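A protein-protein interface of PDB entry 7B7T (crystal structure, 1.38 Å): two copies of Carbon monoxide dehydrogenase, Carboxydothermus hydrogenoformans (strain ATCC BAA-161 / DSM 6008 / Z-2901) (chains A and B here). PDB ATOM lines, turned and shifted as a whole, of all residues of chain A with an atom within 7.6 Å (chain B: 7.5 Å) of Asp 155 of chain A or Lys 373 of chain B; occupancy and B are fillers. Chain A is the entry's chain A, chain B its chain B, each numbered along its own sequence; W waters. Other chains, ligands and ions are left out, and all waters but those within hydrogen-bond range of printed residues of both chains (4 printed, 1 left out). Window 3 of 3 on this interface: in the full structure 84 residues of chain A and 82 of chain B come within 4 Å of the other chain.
OH of Tyr 96 of chain B lies within hydrogen-bond range of OD2 of Asp 153 of chain A, 2.7 Å away.
OD2 of Asp 153 of chain A is in salt-bridge range of NZ of Lys 100 of chain B, at 3.5 Å.
NZ of Lys 373 of chain B lies within salt-bridge range of OD1 of Asp 155 of chain A (3.5 Å).
The guanidinium group (NH1) of Arg 359 of chain B is in salt-bridge range of the side-chain carboxylate (OE2) of Glu 97 of chain B (3.99 Å).
The side-chain carboxylate (OD1) of Asp 153 of chain A lies within hydrogen-bond range of the backbone NH (N) of Glu 156 of chain A.
OH of Tyr 372 of chain B is in hydrogen-bond range of OG1 of Thr 101 of chain B.
The side-chain carboxylate of Asp 371 of chain B is in hydrogen-bond range of the backbone NH of Arg 359 of chain B (3.4 Å).
The backbone carbonyl oxygen (O) of Val 357 of chain B lies within hydrogen-bond range of the backbone NH (N) of Tyr 372 of chain B, at 3.2 Å.
Arg 359 of chain B touches Tyr 154 of chain A (NH1 to CE1, 3.6 Å).
Tyr 154 of chain A touches Tyr 372 of chain B.
Lys 373 of chain B touches Tyr 154 of chain A.
His 185 of chain A touches Tyr 96 of chain B.
Of the printed residues of chain B, Asp 153 of chain A touches Tyr 96 and Lys 100.
Printed residues of chain B within 4 Å of Tyr 154 of chain A: Arg 359 (3.6 Å), Tyr 372 (3.9 Å) and Lys 373 (3.2 Å).
Asp 155 of chain A touches just one residue of chain B: Lys 373 (3.5 Å).
Of the printed residues of chain B, His 185 of chain A touches Tyr 96 (3.6 Å).
Printed residues of chain A within 4 Å of Lys 100 of chain B: Asp 153.
Of the printed residues of chain A, Tyr 372 of chain B touches Tyr 154 (3.9 Å).
Lys 373 of chain B touches just these residues of chain A: Tyr 154 and Asp 155.
The nearest residue of chain B that does not touch Asp 155 of chain A is Lys 100 of chain B (5.9 Å).
The nearest printed residue of chain A that does not touch Tyr 96 of chain B is Glu 156 of chain A (5.9 Å).
Of the 13 printed residues of chain A, 4 touch a printed residue of chain B.
Printed residues of chain A that touch a printed residue of chain B: Asp 153, Tyr 154, Asp 155 and His 185.
Printed residues of chain B that touch a printed residue of chain A: Tyr 96, Lys 100, Arg 359, Tyr 372 and Lys 373.
Among the printed residues, Asp or Glu carboxylates within 4 Å of a Lys or Arg side-chain nitrogen of the other chain: Asp 153 of chain A with Lys 100 of chain B (3.5 Å) and Asp 155 of chain A with Lys 373 of chain B (3.5 Å).
No position is printed for both chains.
Water W4 bridges NZ of Lys 100 of chain B (2.5 Å) and OD2 of Asp 153 of chain A (3.1 Å).
Water W3 lies within hydrogen-bond range of O of Tyr 372 of chain B (2.8 Å), OE2 of Glu 97 of chain B (2.8 Å), OH of Tyr 154 of chain A (2.8 Å) and NH1 of Arg 359 of chain B (3.2 Å).
Water W1 lies within hydrogen-bond range of the backbone carbonyl oxygen (O) of Tyr 372 of chain B, the side-chain hydroxyl (OH) of Tyr 154 of chain A and the guanidinium group (NH1) of Arg 359 of chain B.
Water W2 lies within hydrogen-bond range of the guanidinium group (NH1) of Arg 211 of chain A (3.2 Å) and the guanidinium group (NE) of Arg 359 of chain B (3.4 Å).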
ATOM      1  N   ARG A 152      12.899  11.125  -2.374  1.00  0.00           N
ATOM      2  CA  ARG A 152      13.399  12.047  -1.368  1.00  0.00           C
ATOM      3  C   ARG A 152      12.314  13.065  -0.999  1.00  0.00           C
ATOM      4  O   ARG A 152      11.580  13.543  -1.863  1.00  0.00           O
ATOM      5  CB  ARG A 152      14.606  12.752  -2.018  1.00  0.00           C
ATOM      6  CG  ARG A 152      15.631  13.414  -1.130  1.00  0.00           C
ATOM      7  CD  ARG A 152      16.838  13.871  -1.965  1.00  0.00           C
ATOM      8  NE  ARG A 152      16.451  14.551  -3.195  1.00  0.00           N
ATOM      9  CZ  ARG A 152      15.957  15.782  -3.248  1.00  0.00           C
ATOM     10  NH1 ARG A 152      15.805  16.478  -2.136  1.00  0.00           N
ATOM     11  NH2 ARG A 152      15.615  16.311  -4.415  1.00  0.00           N
ATOM     12  N   ASP A 153      12.181  13.394   0.286  1.00  0.00           N
ATOM     13  CA  ASP A 153      11.109  14.341   0.559  1.00  0.00           C
ATOM     14  C   ASP A 153      11.613  15.772   0.478  1.00  0.00           C
ATOM     15  O   ASP A 153      12.822  16.042   0.355  1.00  0.00           O
ATOM     16  CB  ASP A 153      10.322  14.020   1.844  1.00  0.00           C
ATOM     17  CG  ASP A 153      11.037  14.399   3.115  1.00  0.00           C
ATOM     18  OD1 ASP A 153      12.031  15.125   3.094  1.00  0.00           O
ATOM     19  OD2 ASP A 153      10.559  13.957   4.160  1.00  0.00           O
ATOM     20  N   TYR A 154      10.649  16.696   0.547  1.00  0.00           N
ATOM     21  CA  TYR A 154      10.911  18.117   0.369  1.00  0.00           C
ATOM     22  C   TYR A 154      11.928  18.648   1.344  1.00  0.00           C
ATOM     23  O   TYR A 154      12.374  19.784   1.156  1.00  0.00           O
ATOM     24  CB  TYR A 154       9.598  18.903   0.495  1.00  0.00           C
ATOM     25  CG  TYR A 154       9.281  19.320   1.905  1.00  0.00           C
ATOM     26  CD1 TYR A 154       8.662  18.443   2.779  1.00  0.00           C
ATOM     27  CD2 TYR A 154       9.612  20.587   2.372  1.00  0.00           C
ATOM     28  CE1 TYR A 154       8.365  18.811   4.078  1.00  0.00           C
ATOM     29  CE2 TYR A 154       9.328  20.962   3.674  1.00  0.00           C
ATOM     30  CZ  TYR A 154       8.705  20.066   4.519  1.00  0.00           C
ATOM     31  OH  TYR A 154       8.415  20.419   5.809  1.00  0.00           O
ATOM     32  N   ASP A 155      12.354  17.831   2.308  1.00  0.00           N
ATOM     33  CA  ASP A 155      13.182  18.273   3.417  1.00  0.00           C
ATOM     34  C   ASP A 155      14.489  17.489   3.540  1.00  0.00           C
ATOM     35  O   ASP A 155      15.112  17.519   4.590  1.00  0.00           O
ATOM     36  CB  ASP A 155      12.342  18.180   4.701  1.00  0.00           C
ATOM     37  CG  ASP A 155      13.034  18.759   5.901  1.00  0.00           C
ATOM     38  OD1 ASP A 155      13.263  19.986   5.923  1.00  0.00           O
ATOM     39  OD2 ASP A 155      13.332  17.984   6.833  1.00  0.00           O
ATOM     40  N   GLU A 156      14.980  16.866   2.467  1.00  0.00           N
ATOM     41  CA  GLU A 156      16.193  16.036   2.500  1.00  0.00           C
ATOM     42  C   GLU A 156      17.067  16.348   1.268  1.00  0.00           C
ATOM     43  O   GLU A 156      16.573  16.206   0.154  1.00  0.00           O
ATOM     44  CB  GLU A 156      15.702  14.588   2.498  1.00  0.00           C
ATOM     45  CG  GLU A 156      16.738  13.500   2.419  1.00  0.00           C
ATOM     46  CD  GLU A 156      16.109  12.095   2.550  1.00  0.00           C
ATOM     47  OE1 GLU A 156      14.942  11.898   2.139  1.00  0.00           O
ATOM     48  OE2 GLU A 156      16.780  11.184   3.075  1.00  0.00           O
ATOM     49  N   PRO A 157      18.340  16.783   1.397  1.00  0.00           N
ATOM     50  CA  PRO A 157      19.032  17.367   0.225  1.00  0.00           C
ATOM     51  C   PRO A 157      19.403  16.366  -0.866  1.00  0.00           C
ATOM     52  O   PRO A 157      19.973  15.303  -0.620  1.00  0.00           O
ATOM     53  CB  PRO A 157      20.298  18.001   0.813  1.00  0.00           C
ATOM     54  CG  PRO A 157      20.125  17.958   2.314  1.00  0.00           C
ATOM     55  CD  PRO A 157      19.191  16.832   2.603  1.00  0.00           C
ATOM     56  N   GLY A 158      19.154  16.756  -2.090  1.00  0.00           N
ATOM     57  CA  GLY A 158      19.525  15.903  -3.190  1.00  0.00           C
ATOM     58  C   GLY A 158      20.977  16.057  -3.592  1.00  0.00           C
ATOM     59  O   GLY A 158      21.638  17.035  -3.245  1.00  0.00           O
ATOM     60  N   PRO A 180      13.796  21.453  -5.522  1.00  0.00           N
ATOM     61  CA  PRO A 180      12.715  20.481  -5.391  1.00  0.00           C
ATOM     62  C   PRO A 180      13.022  19.335  -4.434  1.00  0.00           C
ATOM     63  O   PRO A 180      14.170  18.964  -4.196  1.00  0.00           O
ATOM     64  CB  PRO A 180      12.610  19.923  -6.814  1.00  0.00           C
ATOM     65  CG  PRO A 180      13.974  19.955  -7.301  1.00  0.00           C
ATOM     66  CD  PRO A 180      14.523  21.258  -6.789  1.00  0.00           C
ATOM     67  N   ALA A 181      11.941  18.736  -3.944  1.00  0.00           N
ATOM     68  CA  ALA A 181      11.988  17.393  -3.392  1.00  0.00           C
ATOM     69  C   ALA A 181      12.138  16.397  -4.525  1.00  0.00           C
ATOM     70  O   ALA A 181      12.238  16.771  -5.696  1.00  0.00           O
ATOM     71  CB  ALA A 181      10.672  17.081  -2.685  1.00  0.00           C
ATOM     72  N   GLY A 182      12.109  15.116  -4.175  1.00  0.00           N
ATOM     73  CA  GLY A 182      12.028  14.076  -5.166  1.00  0.00           C
ATOM     74  C   GLY A 182      10.733  14.185  -5.949  1.00  0.00           C
ATOM     75  O   GLY A 182       9.712  14.690  -5.459  1.00  0.00           O
ATOM     76  N   HIS A 185       7.299  12.906  -4.335  1.00  0.00           N
ATOM     77  CA  HIS A 185       6.683  13.851  -3.418  1.00  0.00           C
ATOM     78  C   HIS A 185       6.216  15.114  -4.116  1.00  0.00           C
ATOM     79  O   HIS A 185       5.144  15.643  -3.780  1.00  0.00           O
ATOM     80  CB  HIS A 185       7.614  14.203  -2.267  1.00  0.00           C
ATOM     81  CG  HIS A 185       7.563  13.230  -1.146  1.00  0.00           C
ATOM     82  ND1 HIS A 185       6.532  13.198  -0.235  1.00  0.00           N
ATOM     83  CD2 HIS A 185       8.427  12.261  -0.773  1.00  0.00           C
ATOM     84  CE1 HIS A 185       6.764  12.241   0.648  1.00  0.00           C
ATOM     85  NE2 HIS A 185       7.897  11.646   0.327  1.00  0.00           N
ATOM     86  N   GLU A 186       7.005  15.649  -5.054  1.00  0.00           N
ATOM     87  CA  GLU A 186       6.586  16.894  -5.700  1.00  0.00           C
ATOM     88  C   GLU A 186       5.300  16.686  -6.495  1.00  0.00           C
ATOM     89  O   GLU A 186       4.407  17.538  -6.467  1.00  0.00           O
ATOM     90  CB  GLU A 186       7.670  17.521  -6.585  1.00  0.00           C
ATOM     91  CG  GLU A 186       8.897  18.067  -5.843  1.00  0.00           C
ATOM     92  CD  GLU A 186       8.646  19.317  -4.988  1.00  0.00           C
ATOM     93  OE1 GLU A 186       7.543  19.901  -5.032  1.00  0.00           O
ATOM     94  OE2 GLU A 186       9.583  19.732  -4.275  1.00  0.00           O
ATOM     95  N   ARG A 211       8.944  24.106  -9.842  1.00  0.00           N
ATOM     96  CA  ARG A 211       9.557  23.118  -8.954  1.00  0.00           C
ATOM     97  C   ARG A 211       9.381  21.718  -9.498  1.00  0.00           C
ATOM     98  O   ARG A 211      10.298  20.886  -9.461  1.00  0.00           O
ATOM     99  CB  ARG A 211       8.819  23.119  -7.624  1.00  0.00           C
ATOM    100  CG  ARG A 211       8.960  24.315  -6.827  1.00  0.00           C
ATOM    101  CD  ARG A 211       8.125  24.162  -5.590  1.00  0.00           C
ATOM    102  NE  ARG A 211       8.474  22.965  -4.828  1.00  0.00           N
ATOM    103  CZ  ARG A 211       9.297  22.971  -3.795  1.00  0.00           C
ATOM    104  NH1 ARG A 211       9.550  21.843  -3.168  1.00  0.00           N
ATOM    105  NH2 ARG A 211       9.883  24.094  -3.391  1.00  0.00           N
ATOM    106  N   TYR B  96       1.675  10.926   5.362  1.00  0.00           N
ATOM    107  CA  TYR B  96       3.108  11.147   5.499  1.00  0.00           C
ATOM    108  C   TYR B  96       3.404  12.126   6.627  1.00  0.00           C
ATOM    109  O   TYR B  96       4.302  11.893   7.447  1.00  0.00           O
ATOM    110  CB  TYR B  96       3.676  11.647   4.177  1.00  0.00           C
ATOM    111  CG  TYR B  96       5.178  11.658   4.125  1.00  0.00           C
ATOM    112  CD1 TYR B  96       5.885  10.481   3.999  1.00  0.00           C
ATOM    113  CD2 TYR B  96       5.900  12.842   4.167  1.00  0.00           C
ATOM    114  CE1 TYR B  96       7.262  10.476   3.940  1.00  0.00           C
ATOM    115  CE2 TYR B  96       7.298  12.832   4.127  1.00  0.00           C
ATOM    116  CZ  TYR B  96       7.961  11.645   4.003  1.00  0.00           C
ATOM    117  OH  TYR B  96       9.342  11.604   3.933  1.00  0.00           O
ATOM    118  N   GLU B  97       2.643  13.230   6.685  1.00  0.00           N
ATOM    119  CA  GLU B  97       2.844  14.194   7.761  1.00  0.00           C
ATOM    120  C   GLU B  97       2.511  13.600   9.120  1.00  0.00           C
ATOM    121  O   GLU B  97       3.180  13.894  10.108  1.00  0.00           O
ATOM    122  CB  GLU B  97       2.048  15.469   7.496  1.00  0.00           C
ATOM    123  CG  GLU B  97       2.504  16.196   6.239  1.00  0.00           C
ATOM    124  CD  GLU B  97       2.367  17.689   6.332  1.00  0.00           C
ATOM    125  OE1 GLU B  97       1.432  18.159   7.003  1.00  0.00           O
ATOM    126  OE2 GLU B  97       3.192  18.394   5.712  1.00  0.00           O
ATOM    127  N   LYS B 100       5.590  11.426  10.036  1.00  0.00           N
ATOM    128  CA  LYS B 100       6.721  12.245  10.448  1.00  0.00           C
ATOM    129  C   LYS B 100       6.444  12.946  11.766  1.00  0.00           C
ATOM    130  O   LYS B 100       7.368  13.149  12.562  1.00  0.00           O
ATOM    131  CB  LYS B 100       7.039  13.281   9.376  1.00  0.00           C
ATOM    132  CG  LYS B 100       7.555  12.687   8.082  1.00  0.00           C
ATOM    133  CD  LYS B 100       8.957  12.183   8.200  1.00  0.00           C
ATOM    134  CE  LYS B 100       9.806  12.733   7.061  1.00  0.00           C
ATOM    135  NZ  LYS B 100      11.273  12.424   7.177  1.00  0.00           N
ATOM    136  N   THR B 101       5.191  13.340  12.007  1.00  0.00           N
ATOM    137  CA  THR B 101       4.846  13.940  13.289  1.00  0.00           C
ATOM    138  C   THR B 101       5.047  12.957  14.431  1.00  0.00           C
ATOM    139  O   THR B 101       5.591  13.325  15.478  1.00  0.00           O
ATOM    140  CB  THR B 101       3.430  14.521  13.248  1.00  0.00           C
ATOM    141  OG1 THR B 101       3.390  15.560  12.257  1.00  0.00           O
ATOM    142  CG2 THR B 101       3.038  15.123  14.589  1.00  0.00           C
ATOM    143  N   MET B 104       8.922  12.482  14.890  1.00  0.00           N
ATOM    144  CA  MET B 104       9.529  13.634  15.539  1.00  0.00           C
ATOM    145  C   MET B 104       9.064  13.789  16.977  1.00  0.00           C
ATOM    146  O   MET B 104       9.832  14.265  17.814  1.00  0.00           O
ATOM    147  CB  MET B 104       9.218  14.886  14.740  1.00  0.00           C
ATOM    148  CG  MET B 104       9.984  14.917  13.441  1.00  0.00           C
ATOM    149  SD  MET B 104      11.763  15.128  13.622  1.00  0.00           S
ATOM    150  CE  MET B 104      11.770  16.735  14.330  1.00  0.00           C
ATOM    151  N   ASN B 109      10.871  16.249  19.642  1.00  0.00           N
ATOM    152  CA  ASN B 109      10.983  17.516  18.928  1.00  0.00           C
ATOM    153  C   ASN B 109       9.661  18.267  18.759  1.00  0.00           C
ATOM    154  O   ASN B 109       9.633  19.267  18.035  1.00  0.00           O
ATOM    155  CB  ASN B 109      11.609  17.295  17.553  1.00  0.00           C
ATOM    156  CG  ASN B 109      13.001  16.644  17.616  1.00  0.00           C
ATOM    157  OD1 ASN B 109      13.370  15.832  16.749  1.00  0.00           O
ATOM    158  ND2 ASN B 109      13.766  17.001  18.618  1.00  0.00           N
ATOM    159  N   THR B 110       8.574  17.834  19.393  1.00  0.00           N
ATOM    160  CA  THR B 110       7.279  18.481  19.242  1.00  0.00           C
ATOM    161  C   THR B 110       6.619  18.723  20.587  1.00  0.00           C
ATOM    162  O   THR B 110       7.061  18.199  21.612  1.00  0.00           O
ATOM    163  CB  THR B 110       6.340  17.602  18.409  1.00  0.00           C
ATOM    164  OG1 THR B 110       5.873  16.534  19.232  1.00  0.00           O
ATOM    165  CG2 THR B 110       7.036  17.046  17.153  1.00  0.00           C
ATOM    166  N   PRO B 111       5.529  19.503  20.613  1.00  0.00           N
ATOM    167  CA  PRO B 111       4.761  19.670  21.854  1.00  0.00           C
ATOM    168  C   PRO B 111       3.831  18.514  22.171  1.00  0.00           C
ATOM    169  O   PRO B 111       3.137  18.561  23.190  1.00  0.00           O
ATOM    170  CB  PRO B 111       3.952  20.958  21.596  1.00  0.00           C
ATOM    171  CG  PRO B 111       3.933  21.135  20.140  1.00  0.00           C
ATOM    172  CD  PRO B 111       5.109  20.455  19.567  1.00  0.00           C
ATOM    173  N   PHE B 112       3.826  17.476  21.345  1.00  0.00           N
ATOM    174  CA  PHE B 112       2.952  16.330  21.519  1.00  0.00           C
ATOM    175  C   PHE B 112       3.662  15.222  22.289  1.00  0.00           C
ATOM    176  O   PHE B 112       4.850  15.297  22.607  1.00  0.00           O
ATOM    177  CB  PHE B 112       2.536  15.800  20.153  1.00  0.00           C
ATOM    178  CG  PHE B 112       2.101  16.871  19.199  1.00  0.00           C
ATOM    179  CD1 PHE B 112       1.268  17.893  19.615  1.00  0.00           C
ATOM    180  CD2 PHE B 112       2.534  16.864  17.874  1.00  0.00           C
ATOM    181  CE1 PHE B 112       0.850  18.877  18.719  1.00  0.00           C
ATOM    182  CE2 PHE B 112       2.115  17.840  16.982  1.00  0.00           C
ATOM    183  CZ  PHE B 112       1.277  18.852  17.417  1.00  0.00           C
ATOM    184  N   VAL B 263      -1.658  21.532  13.904  1.00  0.00           N
ATOM    185  CA  VAL B 263      -1.618  22.933  14.318  1.00  0.00           C
ATOM    186  C   VAL B 263      -2.705  23.225  15.341  1.00  0.00           C
ATOM    187  O   VAL B 263      -2.481  23.969  16.303  1.00  0.00           O
ATOM    188  CB  VAL B 263      -1.677  23.850  13.081  1.00  0.00           C
ATOM    189  CG1 VAL B 263      -1.864  25.317  13.497  1.00  0.00           C
ATOM    190  CG2 VAL B 263      -0.381  23.689  12.310  1.00  0.00           C
ATOM    191  N   VAL B 357      -1.274  27.538   7.144  1.00  0.00           N
ATOM    192  CA  VAL B 357      -0.318  26.711   7.885  1.00  0.00           C
ATOM    193  C   VAL B 357       0.046  25.466   7.085  1.00  0.00           C
ATOM    194  O   VAL B 357       0.467  24.450   7.645  1.00  0.00           O
ATOM    195  CB  VAL B 357      -0.818  26.391   9.309  1.00  0.00           C
ATOM    196  CG1 VAL B 357      -1.003  27.677  10.107  1.00  0.00           C
ATOM    197  CG2 VAL B 357      -2.123  25.575   9.334  1.00  0.00           C
ATOM    198  N   ARG B 359       1.938  24.448   3.050  1.00  0.00           N
ATOM    199  CA  ARG B 359       2.414  24.880   1.744  1.00  0.00           C
ATOM    200  C   ARG B 359       1.411  24.587   0.645  1.00  0.00           C
ATOM    201  O   ARG B 359       1.510  25.166  -0.444  1.00  0.00           O
ATOM    202  CB  ARG B 359       3.738  24.232   1.389  1.00  0.00           C
ATOM    203  CG  ARG B 359       3.693  22.771   1.273  1.00  0.00           C
ATOM    204  CD  ARG B 359       5.077  22.265   0.909  1.00  0.00           C
ATOM    205  NE  ARG B 359       5.089  20.819   0.768  1.00  0.00           N
ATOM    206  CZ  ARG B 359       5.208  19.971   1.769  1.00  0.00           C
ATOM    207  NH1 ARG B 359       5.349  20.400   3.016  1.00  0.00           N
ATOM    208  NH2 ARG B 359       5.155  18.682   1.514  1.00  0.00           N
ATOM    209  N   LEU B 370       2.776  30.219   7.377  1.00  0.00           N
ATOM    210  CA  LEU B 370       3.539  29.523   8.411  1.00  0.00           C
ATOM    211  C   LEU B 370       3.449  28.023   8.106  1.00  0.00           C
ATOM    212  O   LEU B 370       2.683  27.308   8.740  1.00  0.00           O
ATOM    213  CB  LEU B 370       2.986  29.871   9.785  1.00  0.00           C
ATOM    214  CG  LEU B 370       2.957  31.348  10.183  1.00  0.00           C
ATOM    215  CD1 LEU B 370       2.302  31.518  11.552  1.00  0.00           C
ATOM    216  CD2 LEU B 370       4.364  31.884  10.182  1.00  0.00           C
ATOM    217  N   ASP B 371       4.236  27.572   7.125  1.00  0.00           N
ATOM    218  CA  ASP B 371       4.158  26.201   6.632  1.00  0.00           C
ATOM    219  C   ASP B 371       4.475  25.228   7.773  1.00  0.00           C
ATOM    220  O   ASP B 371       5.435  25.412   8.522  1.00  0.00           O
ATOM    221  CB  ASP B 371       5.195  25.994   5.501  1.00  0.00           C
ATOM    222  CG  ASP B 371       4.858  26.686   4.177  1.00  0.00           C
ATOM    223  OD1 ASP B 371       3.742  27.207   3.998  1.00  0.00           O
ATOM    224  OD2 ASP B 371       5.759  26.665   3.282  1.00  0.00           O
ATOM    225  N   TYR B 372       3.668  24.196   7.919  1.00  0.00           N
ATOM    226  CA  TYR B 372       3.860  23.232   9.004  1.00  0.00           C
ATOM    227  C   TYR B 372       5.147  22.425   8.852  1.00  0.00           C
ATOM    228  O   TYR B 372       5.445  21.899   7.767  1.00  0.00           O
ATOM    229  CB  TYR B 372       2.703  22.245   8.994  1.00  0.00           C
ATOM    230  CG  TYR B 372       2.823  21.135  10.037  1.00  0.00           C
ATOM    231  CD1 TYR B 372       2.681  21.405  11.393  1.00  0.00           C
ATOM    232  CD2 TYR B 372       3.089  19.814   9.664  1.00  0.00           C
ATOM    233  CE1 TYR B 372       2.778  20.421  12.332  1.00  0.00           C
ATOM    234  CE2 TYR B 372       3.168  18.808  10.611  1.00  0.00           C
ATOM    235  CZ  TYR B 372       3.012  19.125  11.950  1.00  0.00           C
ATOM    236  OH  TYR B 372       3.097  18.154  12.913  1.00  0.00           O
ATOM    237  N   LYS B 373       5.883  22.286   9.965  1.00  0.00           N
ATOM    238  CA  LYS B 373       6.890  21.245  10.151  1.00  0.00           C
ATOM    239  C   LYS B 373       6.720  20.820  11.600  1.00  0.00           C
ATOM    240  O   LYS B 373       6.537  21.678  12.462  1.00  0.00           O
ATOM    241  CB  LYS B 373       8.335  21.732   9.951  1.00  0.00           C
ATOM    242  CG  LYS B 373       8.691  22.024   8.510  1.00  0.00           C
ATOM    243  CD  LYS B 373      10.204  22.092   8.279  1.00  0.00           C
ATOM    244  CE  LYS B 373      10.494  23.065   7.140  1.00  0.00           C
ATOM    245  NZ  LYS B 373      11.908  23.132   6.649  1.00  0.00           N
ATOM    246  N   PRO B 374       6.760  19.521  11.902  1.00  0.00           N
ATOM    247  CA  PRO B 374       6.605  19.083  13.310  1.00  0.00           C
ATOM    248  C   PRO B 374       7.506  19.806  14.301  1.00  0.00           C
ATOM    249  O   PRO B 374       7.062  20.210  15.394  1.00  0.00           O
ATOM    250  CB  PRO B 374       6.950  17.588  13.237  1.00  0.00           C
ATOM    251  CG  PRO B 374       6.677  17.204  11.857  1.00  0.00           C
ATOM    252  CD  PRO B 374       6.907  18.385  10.985  1.00  0.00           C
ATOM    253  N   SER B 375       8.777  19.956  13.954  1.00  0.00           N
ATOM    254  CA  SER B 375       9.732  20.568  14.876  1.00  0.00           C
ATOM    255  C   SER B 375       9.539  22.067  15.033  1.00  0.00           C
ATOM    256  O   SER B 375      10.168  22.672  15.914  1.00  0.00           O
ATOM    257  CB  SER B 375      11.153  20.300  14.397  1.00  0.00           C
ATOM    258  OG  SER B 375      11.424  21.015  13.199  1.00  0.00           O
ATOM    259  N   GLU B 376       8.695  22.676  14.209  1.00  0.00           N
ATOM    260  CA  GLU B 376       8.399  24.096  14.298  1.00  0.00           C
ATOM    261  C   GLU B 376       6.980  24.386  14.785  1.00  0.00           C
ATOM    262  O   GLU B 376       6.634  25.553  14.944  1.00  0.00           O
ATOM    263  CB  GLU B 376       8.650  24.781  12.952  1.00  0.00           C
ATOM    264  CG  GLU B 376      10.124  24.738  12.576  1.00  0.00           C
ATOM    265  CD  GLU B 376      10.462  25.206  11.169  1.00  0.00           C
ATOM    266  OE1 GLU B 376       9.590  25.684  10.413  1.00  0.00           O
ATOM    267  OE2 GLU B 376      11.650  25.069  10.812  1.00  0.00           O
ATOM    268  N   VAL B 377       6.146  23.371  15.035  1.00  0.00           N
ATOM    269  CA  VAL B 377       4.738  23.646  15.322  1.00  0.00           C
ATOM    270  C   VAL B 377       4.557  24.410  16.637  1.00  0.00           C
ATOM    271  O   VAL B 377       3.606  25.203  16.773  1.00  0.00           O
ATOM    272  CB  VAL B 377       3.881  22.369  15.221  1.00  0.00           C
ATOM    273  CG1 VAL B 377       4.050  21.484  16.414  1.00  0.00           C
ATOM    274  CG2 VAL B 377       2.406  22.767  15.019  1.00  0.00           C
ATOM    275  N   ARG B 378       5.425  24.192  17.624  1.00  0.00           N
ATOM    276  CA  ARG B 378       5.336  24.969  18.857  1.00  0.00           C
ATOM    277  C   ARG B 378       5.472  26.458  18.553  1.00  0.00           C
ATOM    278  O   ARG B 378       4.661  27.290  18.987  1.00  0.00           O
ATOM    279  CB  ARG B 378       6.441  24.484  19.796  1.00  0.00           C
ATOM    280  CG  ARG B 378       6.446  25.034  21.173  1.00  0.00           C
ATOM    281  CD  ARG B 378       7.739  24.549  21.829  1.00  0.00           C
ATOM    282  NE  ARG B 378       7.628  23.341  22.651  1.00  0.00           N
ATOM    283  CZ  ARG B 378       7.923  22.093  22.279  1.00  0.00           C
ATOM    284  NH1 ARG B 378       8.313  21.783  21.031  1.00  0.00           N
ATOM    285  NH2 ARG B 378       7.796  21.132  23.183  1.00  0.00           N
ATOM    286  N   GLU B 379       6.452  26.805  17.727  1.00  0.00           N
ATOM    287  CA  GLU B 379       6.674  28.199  17.383  1.00  0.00           C
ATOM    288  C   GLU B 379       5.563  28.741  16.473  1.00  0.00           C
ATOM    289  O   GLU B 379       5.153  29.905  16.604  1.00  0.00           O
ATOM    290  CB  GLU B 379       8.058  28.313  16.727  1.00  0.00           C
ATOM    291  CG  GLU B 379       9.275  28.023  17.672  1.00  0.00           C
ATOM    292  CD  GLU B 379       9.476  26.541  18.127  1.00  0.00           C
ATOM    293  OE1 GLU B 379       9.059  25.571  17.429  1.00  0.00           O
ATOM    294  OE2 GLU B 379      10.097  26.349  19.209  1.00  0.00           O
ATOM    295  N   ILE B 380       5.062  27.918  15.543  1.00  0.00           N
ATOM    296  CA  ILE B 380       3.940  28.325  14.688  1.00  0.00           C
ATOM    297  C   ILE B 380       2.727  28.688  15.544  1.00  0.00           C
ATOM    298  O   ILE B 380       2.092  29.731  15.348  1.00  0.00           O
ATOM    299  CB  ILE B 380       3.593  27.218  13.670  1.00  0.00           C
ATOM    300  CG1 ILE B 380       4.702  27.089  12.627  1.00  0.00           C
ATOM    301  CG2 ILE B 380       2.232  27.462  12.995  1.00  0.00           C
ATOM    302  CD1 ILE B 380       4.638  25.804  11.805  1.00  0.00           C
HETATM  303  O   HOH W   1       6.327  22.742   5.219  1.00  0.00           O
HETATM  304  O   HOH W   2       8.044  21.958  -0.387  1.00  0.00           O
HETATM  305  O   HOH W   3       5.689  19.680   6.133  1.00  0.00           O
HETATM  306  O   HOH W   4      12.907  12.307   5.251  1.00  0.00           O
